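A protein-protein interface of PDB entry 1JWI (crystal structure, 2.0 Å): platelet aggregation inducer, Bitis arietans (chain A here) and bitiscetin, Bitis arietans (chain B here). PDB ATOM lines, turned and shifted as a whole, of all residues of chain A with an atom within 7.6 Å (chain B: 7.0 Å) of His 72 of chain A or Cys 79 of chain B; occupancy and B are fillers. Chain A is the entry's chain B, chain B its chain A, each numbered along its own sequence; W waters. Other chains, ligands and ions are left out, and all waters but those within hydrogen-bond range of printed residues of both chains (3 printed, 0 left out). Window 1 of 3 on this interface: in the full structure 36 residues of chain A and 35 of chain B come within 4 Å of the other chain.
His 72 of chain A touches just one residue of chain B: Cys 79 (3.9 Å). Of chain A, only His 72 (3.9 Å), Ile 76 (3.9 Å) and Cys 77 (2.0 Å) come within 4 Å of Cys 79 of chain B. Of the printed residues of chain A, Asp 72 of chain B touches Pro 78 and Leu 79. Printed residues of chain B within 4 Å of Ile 76 of chain A: Cys 79 (3.9 Å). Of the printed residues of chain A, Val 89 of chain B touches Leu 70 (3.8 Å). Ile 97 of chain A touches none of the printed residues of chain B. Gln 82 of chain B touches none of the printed residues of chain A. The nearest residue of chain A that does not touch Cys 79 of chain B is Pro 78 of chain A (4.6 Å).
CG of Leu 70 of chain A touches NE2 of Gln 78 of chain B, at 3.7 Å. CG2 of Val 89 of chain B touches CD1 of Leu 70 of chain A, 3.8 Å away. O of Ser 71 of chain A touches OG of Ser 80 of chain B (3.9 Å). CE1 of His 72 of chain A touches CB of Cys 79 of chain B, at 3.9 Å. SG of Cys 79 of chain B touches O of Ile 76 of chain A (3.9 Å). CG of Pro 78 of chain A touches OD2 of Asp 72 of chain B (3.6 Å). Ser 74 of chain B touches Pro 78 of chain A (N to CG, 3.4 Å). Leu 79 of chain A touches Asp 72 of chain B (CD2 to CA, 3.7 Å). CZ of Phe 99 of chain A touches CB of Gln 78 of chain B, 3.7 Å away.
OD2 of Asp 72 of chain B is in hydrogen-bond range of OG of Ser 74 of chain B (2.7 Å). The backbone carbonyl oxygen (O) of Ser 74 of chain B is in hydrogen-bond range of the side-chain amino group (NZ) of Lys 99 of chain B. The side-chain amide nitrogen (NE2) of Gln 78 of chain B sits close to the backbone NH (N) of Ser 80 of chain B. The side-chain hydroxyl (OG) of Ser 80 of chain B sits at hydrogen-bond distance from the backbone carbonyl oxygen (O) of Gln 82 of chain B. OG of Ser 71 of chain A sits at hydrogen-bond distance from O of Ile 97 of chain A. The side-chain hydroxyl (OG) of Ser 71 of chain A lies within hydrogen-bond range of the side-chain sulfur (SG) of Cys 98 of chain A.
The side-chain sulfur (SG) of Cys 79 of chain B forms a disulfide with the side-chain sulfur (SG) of Cys 77 of chain A, at 2.0 Å.
Water W2 bridges NE2 of His 72 of chain A and N of Cys 79 of chain B. Water W3 lies within hydrogen-bond range of the backbone carbonyl oxygen of Gln 82 of chain B, the side-chain hydroxyl of Ser 80 of chain B and the backbone NH of Ser 71 of chain A. Water W1 bridges the backbone carbonyl oxygen (O) of Cys 79 of chain B (3.2 Å) and the backbone carbonyl oxygen (O) of Ile 76 of chain A (3.5 Å).
Of the 19 printed residues of chain A, 8 touch a printed residue of chain B. Of the 12 printed residues of chain B, 6 touch a printed residue of chain A. Hydrophobic or aromatic side chains of chain B that line the printed part of chain A: Val 89. Among the printed residues, no Asp or Glu carboxylate lies within 4 Å of a Lys or Arg side-chain nitrogen of the other chain.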
ATOM      1  N   TRP A  25      33.408  -5.308   2.391  1.00  0.00           N
ATOM      2  CA  TRP A  25      32.416  -5.846   3.316  1.00  0.00           C
ATOM      3  C   TRP A  25      31.908  -7.194   2.821  1.00  0.00           C
ATOM      4  O   TRP A  25      31.967  -8.187   3.546  1.00  0.00           O
ATOM      5  CB  TRP A  25      31.240  -4.882   3.462  1.00  0.00           C
ATOM      6  CG  TRP A  25      30.257  -5.285   4.527  1.00  0.00           C
ATOM      7  CD1 TRP A  25      30.307  -4.979   5.857  1.00  0.00           C
ATOM      8  CD2 TRP A  25      29.078  -6.071   4.341  1.00  0.00           C
ATOM      9  NE1 TRP A  25      29.226  -5.527   6.517  1.00  0.00           N
ATOM     10  CE2 TRP A  25      28.457  -6.204   5.607  1.00  0.00           C
ATOM     11  CE3 TRP A  25      28.484  -6.679   3.228  1.00  0.00           C
ATOM     12  CZ2 TRP A  25      27.270  -6.918   5.784  1.00  0.00           C
ATOM     13  CZ3 TRP A  25      27.303  -7.389   3.405  1.00  0.00           C
ATOM     14  CH2 TRP A  25      26.710  -7.502   4.678  1.00  0.00           C
ATOM     15  N   LEU A  70      26.539  -5.408   9.552  1.00  0.00           N
ATOM     16  CA  LEU A  70      25.382  -4.548   9.336  1.00  0.00           C
ATOM     17  C   LEU A  70      25.505  -3.835   7.986  1.00  0.00           C
ATOM     18  O   LEU A  70      26.520  -3.186   7.708  1.00  0.00           O
ATOM     19  CB  LEU A  70      25.320  -3.522  10.469  1.00  0.00           C
ATOM     20  CG  LEU A  70      23.999  -3.024  11.035  1.00  0.00           C
ATOM     21  CD1 LEU A  70      23.126  -4.205  11.498  1.00  0.00           C
ATOM     22  CD2 LEU A  70      24.317  -2.077  12.197  1.00  0.00           C
ATOM     23  N   SER A  71      24.468  -3.948   7.163  1.00  0.00           N
ATOM     24  CA  SER A  71      24.454  -3.328   5.841  1.00  0.00           C
ATOM     25  C   SER A  71      23.022  -3.262   5.315  1.00  0.00           C
ATOM     26  O   SER A  71      22.199  -4.105   5.655  1.00  0.00           O
ATOM     27  CB  SER A  71      25.308  -4.153   4.869  1.00  0.00           C
ATOM     28  OG  SER A  71      25.237  -3.630   3.556  1.00  0.00           O
ATOM     29  N   HIS A  72      22.726  -2.268   4.483  1.00  0.00           N
ATOM     30  CA  HIS A  72      21.381  -2.143   3.932  1.00  0.00           C
ATOM     31  C   HIS A  72      21.365  -1.236   2.708  1.00  0.00           C
ATOM     32  O   HIS A  72      22.319  -0.497   2.465  1.00  0.00           O
ATOM     33  CB  HIS A  72      20.437  -1.578   4.996  1.00  0.00           C
ATOM     34  CG  HIS A  72      20.712  -0.148   5.354  1.00  0.00           C
ATOM     35  ND1 HIS A  72      20.259   0.910   4.598  1.00  0.00           N
ATOM     36  CD2 HIS A  72      21.407   0.395   6.383  1.00  0.00           C
ATOM     37  CE1 HIS A  72      20.660   2.047   5.144  1.00  0.00           C
ATOM     38  NE2 HIS A  72      21.359   1.760   6.229  1.00  0.00           N
ATOM     39  N   PHE A  73      20.293  -1.331   1.923  1.00  0.00           N
ATOM     40  CA  PHE A  73      20.097  -0.481   0.745  1.00  0.00           C
ATOM     41  C   PHE A  73      18.907   0.396   1.133  1.00  0.00           C
ATOM     42  O   PHE A  73      18.054  -0.038   1.900  1.00  0.00           O
ATOM     43  CB  PHE A  73      19.699  -1.289  -0.498  1.00  0.00           C
ATOM     44  CG  PHE A  73      20.766  -2.195  -1.020  1.00  0.00           C
ATOM     45  CD1 PHE A  73      21.040  -3.407  -0.396  1.00  0.00           C
ATOM     46  CD2 PHE A  73      21.468  -1.859  -2.175  1.00  0.00           C
ATOM     47  CE1 PHE A  73      21.996  -4.278  -0.918  1.00  0.00           C
ATOM     48  CE2 PHE A  73      22.426  -2.723  -2.708  1.00  0.00           C
ATOM     49  CZ  PHE A  73      22.691  -3.934  -2.081  1.00  0.00           C
ATOM     50  N   TRP A  74      18.836   1.615   0.606  1.00  0.00           N
ATOM     51  CA  TRP A  74      17.722   2.502   0.936  1.00  0.00           C
ATOM     52  C   TRP A  74      16.400   1.877   0.500  1.00  0.00           C
ATOM     53  O   TRP A  74      15.369   2.078   1.130  1.00  0.00           O
ATOM     54  CB  TRP A  74      17.911   3.872   0.267  1.00  0.00           C
ATOM     55  CG  TRP A  74      19.025   4.654   0.886  1.00  0.00           C
ATOM     56  CD1 TRP A  74      20.120   5.168   0.259  1.00  0.00           C
ATOM     57  CD2 TRP A  74      19.156   4.996   2.270  1.00  0.00           C
ATOM     58  NE1 TRP A  74      20.934   5.811   1.169  1.00  0.00           N
ATOM     59  CE2 TRP A  74      20.365   5.719   2.412  1.00  0.00           C
ATOM     60  CE3 TRP A  74      18.370   4.761   3.406  1.00  0.00           C
ATOM     61  CZ2 TRP A  74      20.807   6.208   3.643  1.00  0.00           C
ATOM     62  CZ3 TRP A  74      18.806   5.249   4.634  1.00  0.00           C
ATOM     63  CH2 TRP A  74      20.018   5.966   4.742  1.00  0.00           C
ATOM     64  N   ARG A  75      16.455   1.113  -0.583  1.00  0.00           N
ATOM     65  CA  ARG A  75      15.291   0.433  -1.137  1.00  0.00           C
ATOM     66  C   ARG A  75      14.528  -0.355  -0.081  1.00  0.00           C
ATOM     67  O   ARG A  75      13.327  -0.558  -0.211  1.00  0.00           O
ATOM     68  CB  ARG A  75      15.737  -0.523  -2.246  1.00  0.00           C
ATOM     69  CG  ARG A  75      14.650  -1.437  -2.794  1.00  0.00           C
ATOM     70  CD  ARG A  75      15.211  -2.832  -3.049  1.00  0.00           C
ATOM     71  NE  ARG A  75      16.481  -2.797  -3.776  1.00  0.00           N
ATOM     72  CZ  ARG A  75      17.656  -3.160  -3.268  1.00  0.00           C
ATOM     73  NH1 ARG A  75      17.737  -3.592  -2.020  1.00  0.00           N
ATOM     74  NH2 ARG A  75      18.751  -3.087  -4.013  1.00  0.00           N
ATOM     75  N   ILE A  76      15.220  -0.798   0.966  1.00  0.00           N
ATOM     76  CA  ILE A  76      14.571  -1.582   2.010  1.00  0.00           C
ATOM     77  C   ILE A  76      14.271  -0.825   3.302  1.00  0.00           C
ATOM     78  O   ILE A  76      13.949  -1.439   4.317  1.00  0.00           O
ATOM     79  CB  ILE A  76      15.404  -2.857   2.345  1.00  0.00           C
ATOM     80  CG1 ILE A  76      16.831  -2.475   2.742  1.00  0.00           C
ATOM     81  CG2 ILE A  76      15.427  -3.793   1.145  1.00  0.00           C
ATOM     82  CD1 ILE A  76      17.764  -3.668   2.955  1.00  0.00           C
ATOM     83  N   CYS A  77      14.355   0.503   3.263  1.00  0.00           N
ATOM     84  CA  CYS A  77      14.068   1.316   4.443  1.00  0.00           C
ATOM     85  C   CYS A  77      12.730   2.038   4.296  1.00  0.00           C
ATOM     86  O   CYS A  77      12.326   2.405   3.200  1.00  0.00           O
ATOM     87  CB  CYS A  77      15.198   2.321   4.681  1.00  0.00           C
ATOM     88  SG  CYS A  77      16.791   1.450   4.672  1.00  0.00           S
ATOM     89  N   PRO A  78      12.022   2.235   5.414  1.00  0.00           N
ATOM     90  CA  PRO A  78      10.726   2.914   5.388  1.00  0.00           C
ATOM     91  C   PRO A  78      10.854   4.423   5.159  1.00  0.00           C
ATOM     92  O   PRO A  78      10.655   5.212   6.076  1.00  0.00           O
ATOM     93  CB  PRO A  78      10.136   2.571   6.759  1.00  0.00           C
ATOM     94  CG  PRO A  78      11.365   2.518   7.630  1.00  0.00           C
ATOM     95  CD  PRO A  78      12.343   1.751   6.769  1.00  0.00           C
ATOM     96  N   LEU A  79      11.197   4.824   3.945  1.00  0.00           N
ATOM     97  CA  LEU A  79      11.327   6.253   3.656  1.00  0.00           C
ATOM     98  C   LEU A  79       9.951   6.815   3.327  1.00  0.00           C
ATOM     99  O   LEU A  79       9.257   6.287   2.460  1.00  0.00           O
ATOM    100  CB  LEU A  79      12.272   6.477   2.479  1.00  0.00           C
ATOM    101  CG  LEU A  79      13.654   5.832   2.589  1.00  0.00           C
ATOM    102  CD1 LEU A  79      14.452   6.200   1.347  1.00  0.00           C
ATOM    103  CD2 LEU A  79      14.369   6.291   3.852  1.00  0.00           C
ATOM    104  N   ASP A  94      21.863   4.019  -5.029  1.00  0.00           N
ATOM    105  CA  ASP A  94      21.314   2.667  -5.013  1.00  0.00           C
ATOM    106  C   ASP A  94      22.400   1.693  -4.570  1.00  0.00           C
ATOM    107  O   ASP A  94      22.292   0.481  -4.755  1.00  0.00           O
ATOM    108  CB  ASP A  94      20.769   2.278  -6.393  1.00  0.00           C
ATOM    109  CG  ASP A  94      21.706   2.655  -7.519  1.00  0.00           C
ATOM    110  OD1 ASP A  94      22.890   2.265  -7.464  1.00  0.00           O
ATOM    111  OD2 ASP A  94      21.255   3.342  -8.463  1.00  0.00           O
ATOM    112  N   GLU A  95      23.451   2.248  -3.976  1.00  0.00           N
ATOM    113  CA  GLU A  95      24.570   1.459  -3.475  1.00  0.00           C
ATOM    114  C   GLU A  95      24.291   1.147  -1.999  1.00  0.00           C
ATOM    115  O   GLU A  95      23.679   1.946  -1.293  1.00  0.00           O
ATOM    116  CB  GLU A  95      25.863   2.267  -3.612  1.00  0.00           C
ATOM    117  CG  GLU A  95      27.090   1.468  -4.025  1.00  0.00           C
ATOM    118  CD  GLU A  95      26.963   0.859  -5.415  1.00  0.00           C
ATOM    119  OE1 GLU A  95      28.010   0.543  -6.020  1.00  0.00           O
ATOM    120  OE2 GLU A  95      25.824   0.686  -5.900  1.00  0.00           O
ATOM    121  N   PRO A  96      24.734  -0.020  -1.515  1.00  0.00           N
ATOM    122  CA  PRO A  96      24.491  -0.362  -0.112  1.00  0.00           C
ATOM    123  C   PRO A  96      25.298   0.497   0.855  1.00  0.00           C
ATOM    124  O   PRO A  96      26.269   1.148   0.466  1.00  0.00           O
ATOM    125  CB  PRO A  96      24.896  -1.830  -0.044  1.00  0.00           C
ATOM    126  CG  PRO A  96      26.033  -1.890  -1.013  1.00  0.00           C
ATOM    127  CD  PRO A  96      25.510  -1.077  -2.186  1.00  0.00           C
ATOM    128  N   ILE A  97      24.875   0.493   2.114  1.00  0.00           N
ATOM    129  CA  ILE A  97      25.544   1.229   3.181  1.00  0.00           C
ATOM    130  C   ILE A  97      26.120   0.151   4.096  1.00  0.00           C
ATOM    131  O   ILE A  97      25.428  -0.802   4.422  1.00  0.00           O
ATOM    132  CB  ILE A  97      24.541   2.074   4.000  1.00  0.00           C
ATOM    133  CG1 ILE A  97      23.806   3.066   3.092  1.00  0.00           C
ATOM    134  CG2 ILE A  97      25.267   2.800   5.124  1.00  0.00           C
ATOM    135  CD1 ILE A  97      24.705   4.078   2.437  1.00  0.00           C
ATOM    136  N   CYS A  98      27.384   0.282   4.483  1.00  0.00           N
ATOM    137  CA  CYS A  98      28.012  -0.698   5.369  1.00  0.00           C
ATOM    138  C   CYS A  98      28.541   0.008   6.619  1.00  0.00           C
ATOM    139  O   CYS A  98      28.760   1.220   6.605  1.00  0.00           O
ATOM    140  CB  CYS A  98      29.146  -1.443   4.645  1.00  0.00           C
ATOM    141  SG  CYS A  98      28.494  -2.514   3.329  1.00  0.00           S
ATOM    142  N   PHE A  99      28.724  -0.746   7.700  1.00  0.00           N
ATOM    143  CA  PHE A  99      29.209  -0.165   8.944  1.00  0.00           C
ATOM    144  C   PHE A  99      30.476  -0.826   9.473  1.00  0.00           C
ATOM    145  O   PHE A  99      30.669  -2.036   9.338  1.00  0.00           O
ATOM    146  CB  PHE A  99      28.144  -0.260  10.047  1.00  0.00           C
ATOM    147  CG  PHE A  99      26.947   0.625   9.834  1.00  0.00           C
ATOM    148  CD1 PHE A  99      25.906   0.234   8.993  1.00  0.00           C
ATOM    149  CD2 PHE A  99      26.870   1.864  10.467  1.00  0.00           C
ATOM    150  CE1 PHE A  99      24.798   1.070   8.783  1.00  0.00           C
ATOM    151  CE2 PHE A  99      25.773   2.704  10.265  1.00  0.00           C
ATOM    152  CZ  PHE A  99      24.735   2.307   9.423  1.00  0.00           C
ATOM    153  N   GLN A 110      29.148   4.771   9.337  1.00  0.00           N
ATOM    154  CA  GLN A 110      28.786   4.411   7.966  1.00  0.00           C
ATOM    155  C   GLN A 110      30.061   4.435   7.129  1.00  0.00           C
ATOM    156  O   GLN A 110      30.889   5.333   7.285  1.00  0.00           O
ATOM    157  CB  GLN A 110      27.794   5.422   7.383  1.00  0.00           C
ATOM    158  CG  GLN A 110      26.333   5.035   7.490  1.00  0.00           C
ATOM    159  CD  GLN A 110      25.420   6.057   6.824  1.00  0.00           C
ATOM    160  OE1 GLN A 110      25.789   6.682   5.828  1.00  0.00           O
ATOM    161  NE2 GLN A 110      24.217   6.219   7.363  1.00  0.00           N
ATOM    162  N   CYS A 113      30.987   0.483   1.175  1.00  0.00           N
ATOM    163  CA  CYS A 113      31.161  -0.961   1.163  1.00  0.00           C
ATOM    164  C   CYS A 113      32.293  -1.546   0.316  1.00  0.00           C
ATOM    165  O   CYS A 113      32.835  -2.596   0.664  1.00  0.00           O
ATOM    166  CB  CYS A 113      29.858  -1.629   0.748  1.00  0.00           C
ATOM    167  SG  CYS A 113      28.376  -1.253   1.740  1.00  0.00           S
ATOM    168  N   ASP B  72      13.689   8.697   7.143  1.00  0.00           N
ATOM    169  CA  ASP B  72      13.731   7.260   7.399  1.00  0.00           C
ATOM    170  C   ASP B  72      12.947   7.076   8.699  1.00  0.00           C
ATOM    171  O   ASP B  72      13.411   7.467   9.765  1.00  0.00           O
ATOM    172  CB  ASP B  72      15.181   6.790   7.578  1.00  0.00           C
ATOM    173  CG  ASP B  72      15.281   5.334   8.047  1.00  0.00           C
ATOM    174  OD1 ASP B  72      16.410   4.874   8.315  1.00  0.00           O
ATOM    175  OD2 ASP B  72      14.239   4.654   8.148  1.00  0.00           O
ATOM    176  N   SER B  74      12.228   4.315  10.386  1.00  0.00           N
ATOM    177  CA  SER B  74      12.506   3.159  11.237  1.00  0.00           C
ATOM    178  C   SER B  74      12.785   3.628  12.666  1.00  0.00           C
ATOM    179  O   SER B  74      13.307   4.718  12.876  1.00  0.00           O
ATOM    180  CB  SER B  74      13.673   2.328  10.677  1.00  0.00           C
ATOM    181  OG  SER B  74      14.781   3.128  10.320  1.00  0.00           O
ATOM    182  N   THR B  76      14.804   2.159  14.820  1.00  0.00           N
ATOM    183  CA  THR B  76      16.195   1.876  15.179  1.00  0.00           C
ATOM    184  C   THR B  76      17.107   3.037  14.755  1.00  0.00           C
ATOM    185  O   THR B  76      16.680   3.928  14.021  1.00  0.00           O
ATOM    186  CB  THR B  76      16.674   0.561  14.511  1.00  0.00           C
ATOM    187  OG1 THR B  76      16.154   0.476  13.180  1.00  0.00           O
ATOM    188  CG2 THR B  76      16.200  -0.643  15.306  1.00  0.00           C
ATOM    189  N   GLN B  77      18.349   3.035  15.230  1.00  0.00           N
ATOM    190  CA  GLN B  77      19.299   4.092  14.884  1.00  0.00           C
ATOM    191  C   GLN B  77      19.633   4.056  13.394  1.00  0.00           C
ATOM    192  O   GLN B  77      19.769   5.096  12.756  1.00  0.00           O
ATOM    193  CB  GLN B  77      20.571   3.955  15.727  1.00  0.00           C
ATOM    194  CG  GLN B  77      20.373   4.370  17.183  1.00  0.00           C
ATOM    195  CD  GLN B  77      21.568   4.049  18.068  1.00  0.00           C
ATOM    196  OE1 GLN B  77      22.712   4.045  17.617  1.00  0.00           O
ATOM    197  NE2 GLN B  77      21.303   3.795  19.347  1.00  0.00           N
ATOM    198  N   GLN B  78      19.783   2.852  12.851  1.00  0.00           N
ATOM    199  CA  GLN B  78      20.047   2.691  11.430  1.00  0.00           C
ATOM    200  C   GLN B  78      18.912   1.825  10.884  1.00  0.00           C
ATOM    201  O   GLN B  78      18.075   1.337  11.648  1.00  0.00           O
ATOM    202  CB  GLN B  78      21.441   2.083  11.169  1.00  0.00           C
ATOM    203  CG  GLN B  78      21.809   0.854  11.986  1.00  0.00           C
ATOM    204  CD  GLN B  78      21.093  -0.396  11.526  1.00  0.00           C
ATOM    205  OE1 GLN B  78      20.409  -1.055  12.315  1.00  0.00           O
ATOM    206  NE2 GLN B  78      21.253  -0.741  10.249  1.00  0.00           N
ATOM    207  N   CYS B  79      18.882   1.627   9.575  1.00  0.00           N
ATOM    208  CA  CYS B  79      17.786   0.903   8.953  1.00  0.00           C
ATOM    209  C   CYS B  79      17.698  -0.629   8.972  1.00  0.00           C
ATOM    210  O   CYS B  79      16.603  -1.183   8.869  1.00  0.00           O
ATOM    211  CB  CYS B  79      17.655   1.420   7.526  1.00  0.00           C
ATOM    212  SG  CYS B  79      16.746   0.360   6.387  1.00  0.00           S
ATOM    213  N   SER B  80      18.816  -1.325   9.112  1.00  0.00           N
ATOM    214  CA  SER B  80      18.752  -2.784   9.110  1.00  0.00           C
ATOM    215  C   SER B  80      18.096  -3.379  10.359  1.00  0.00           C
ATOM    216  O   SER B  80      18.509  -3.097  11.481  1.00  0.00           O
ATOM    217  CB  SER B  80      20.150  -3.373   8.955  1.00  0.00           C
ATOM    218  OG  SER B  80      20.070  -4.783   8.912  1.00  0.00           O
ATOM    219  N   PRO B  81      17.056  -4.207  10.178  1.00  0.00           N
ATOM    220  CA  PRO B  81      16.388  -4.816  11.332  1.00  0.00           C
ATOM    221  C   PRO B  81      17.112  -6.071  11.846  1.00  0.00           C
ATOM    222  O   PRO B  81      16.815  -6.558  12.937  1.00  0.00           O
ATOM    223  CB  PRO B  81      14.993  -5.111  10.799  1.00  0.00           C
ATOM    224  CG  PRO B  81      15.269  -5.472   9.366  1.00  0.00           C
ATOM    225  CD  PRO B  81      16.259  -4.402   8.951  1.00  0.00           C
ATOM    226  N   GLN B  82      18.069  -6.583  11.068  1.00  0.00           N
ATOM    227  CA  GLN B  82      18.822  -7.768  11.478  1.00  0.00           C
ATOM    228  C   GLN B  82      20.282  -7.788  11.002  1.00  0.00           C
ATOM    229  O   GLN B  82      20.641  -7.128  10.020  1.00  0.00           O
ATOM    230  CB  GLN B  82      18.111  -9.041  11.000  1.00  0.00           C
ATOM    231  CG  GLN B  82      16.787  -9.294  11.696  1.00  0.00           C
ATOM    232  CD  GLN B  82      16.271 -10.707  11.492  1.00  0.00           C
ATOM    233  OE1 GLN B  82      15.325 -11.133  12.152  1.00  0.00           O
ATOM    234  NE2 GLN B  82      16.892 -11.440  10.579  1.00  0.00           N
ATOM    235  N   VAL B  89      18.321  -6.751  15.519  1.00  0.00           N
ATOM    236  CA  VAL B  89      19.094  -5.599  15.935  1.00  0.00           C
ATOM    237  C   VAL B  89      18.327  -4.975  17.096  1.00  0.00           C
ATOM    238  O   VAL B  89      17.235  -4.442  16.910  1.00  0.00           O
ATOM    239  CB  VAL B  89      19.234  -4.573  14.800  1.00  0.00           C
ATOM    240  CG1 VAL B  89      19.871  -3.311  15.334  1.00  0.00           C
ATOM    241  CG2 VAL B  89      20.090  -5.149  13.665  1.00  0.00           C
ATOM    242  N   GLU B  92      22.225  -0.973  19.765  1.00  0.00           N
ATOM    243  CA  GLU B  92      22.820  -0.181  18.677  1.00  0.00           C
ATOM    244  C   GLU B  92      23.736   0.896  19.251  1.00  0.00           C
ATOM    245  O   GLU B  92      23.455   1.451  20.311  1.00  0.00           O
ATOM    246  CB  GLU B  92      21.740   0.513  17.835  1.00  0.00           C
ATOM    247  CG  GLU B  92      20.953  -0.402  16.911  1.00  0.00           C
ATOM    248  CD  GLU B  92      20.003   0.375  16.026  1.00  0.00           C
ATOM    249  OE1 GLU B  92      19.034   0.953  16.563  1.00  0.00           O
ATOM    250  OE2 GLU B  92      20.237   0.416  14.795  1.00  0.00           O
ATOM    251  N   LYS B  99      19.011  10.114   9.531  1.00  0.00           N
ATOM    252  CA  LYS B  99      17.693   9.656   9.092  1.00  0.00           C
ATOM    253  C   LYS B  99      16.854  10.652   8.303  1.00  0.00           C
ATOM    254  O   LYS B  99      15.762  10.316   7.847  1.00  0.00           O
ATOM    255  CB  LYS B  99      16.912   9.153  10.315  1.00  0.00           C
ATOM    256  CG  LYS B  99      17.711   8.114  11.102  1.00  0.00           C
ATOM    257  CD  LYS B  99      17.043   7.689  12.388  1.00  0.00           C
ATOM    258  CE  LYS B  99      15.960   6.662  12.144  1.00  0.00           C
ATOM    259  NZ  LYS B  99      15.398   6.213  13.442  1.00  0.00           N
HETATM  260  O   HOH W   1      13.646  -1.448   7.796  1.00  0.00           O
HETATM  261  O   HOH W   2      20.816   3.585   8.256  1.00  0.00           O
HETATM  262  O   HOH W   3      22.755  -6.662   8.226  1.00  0.00           O
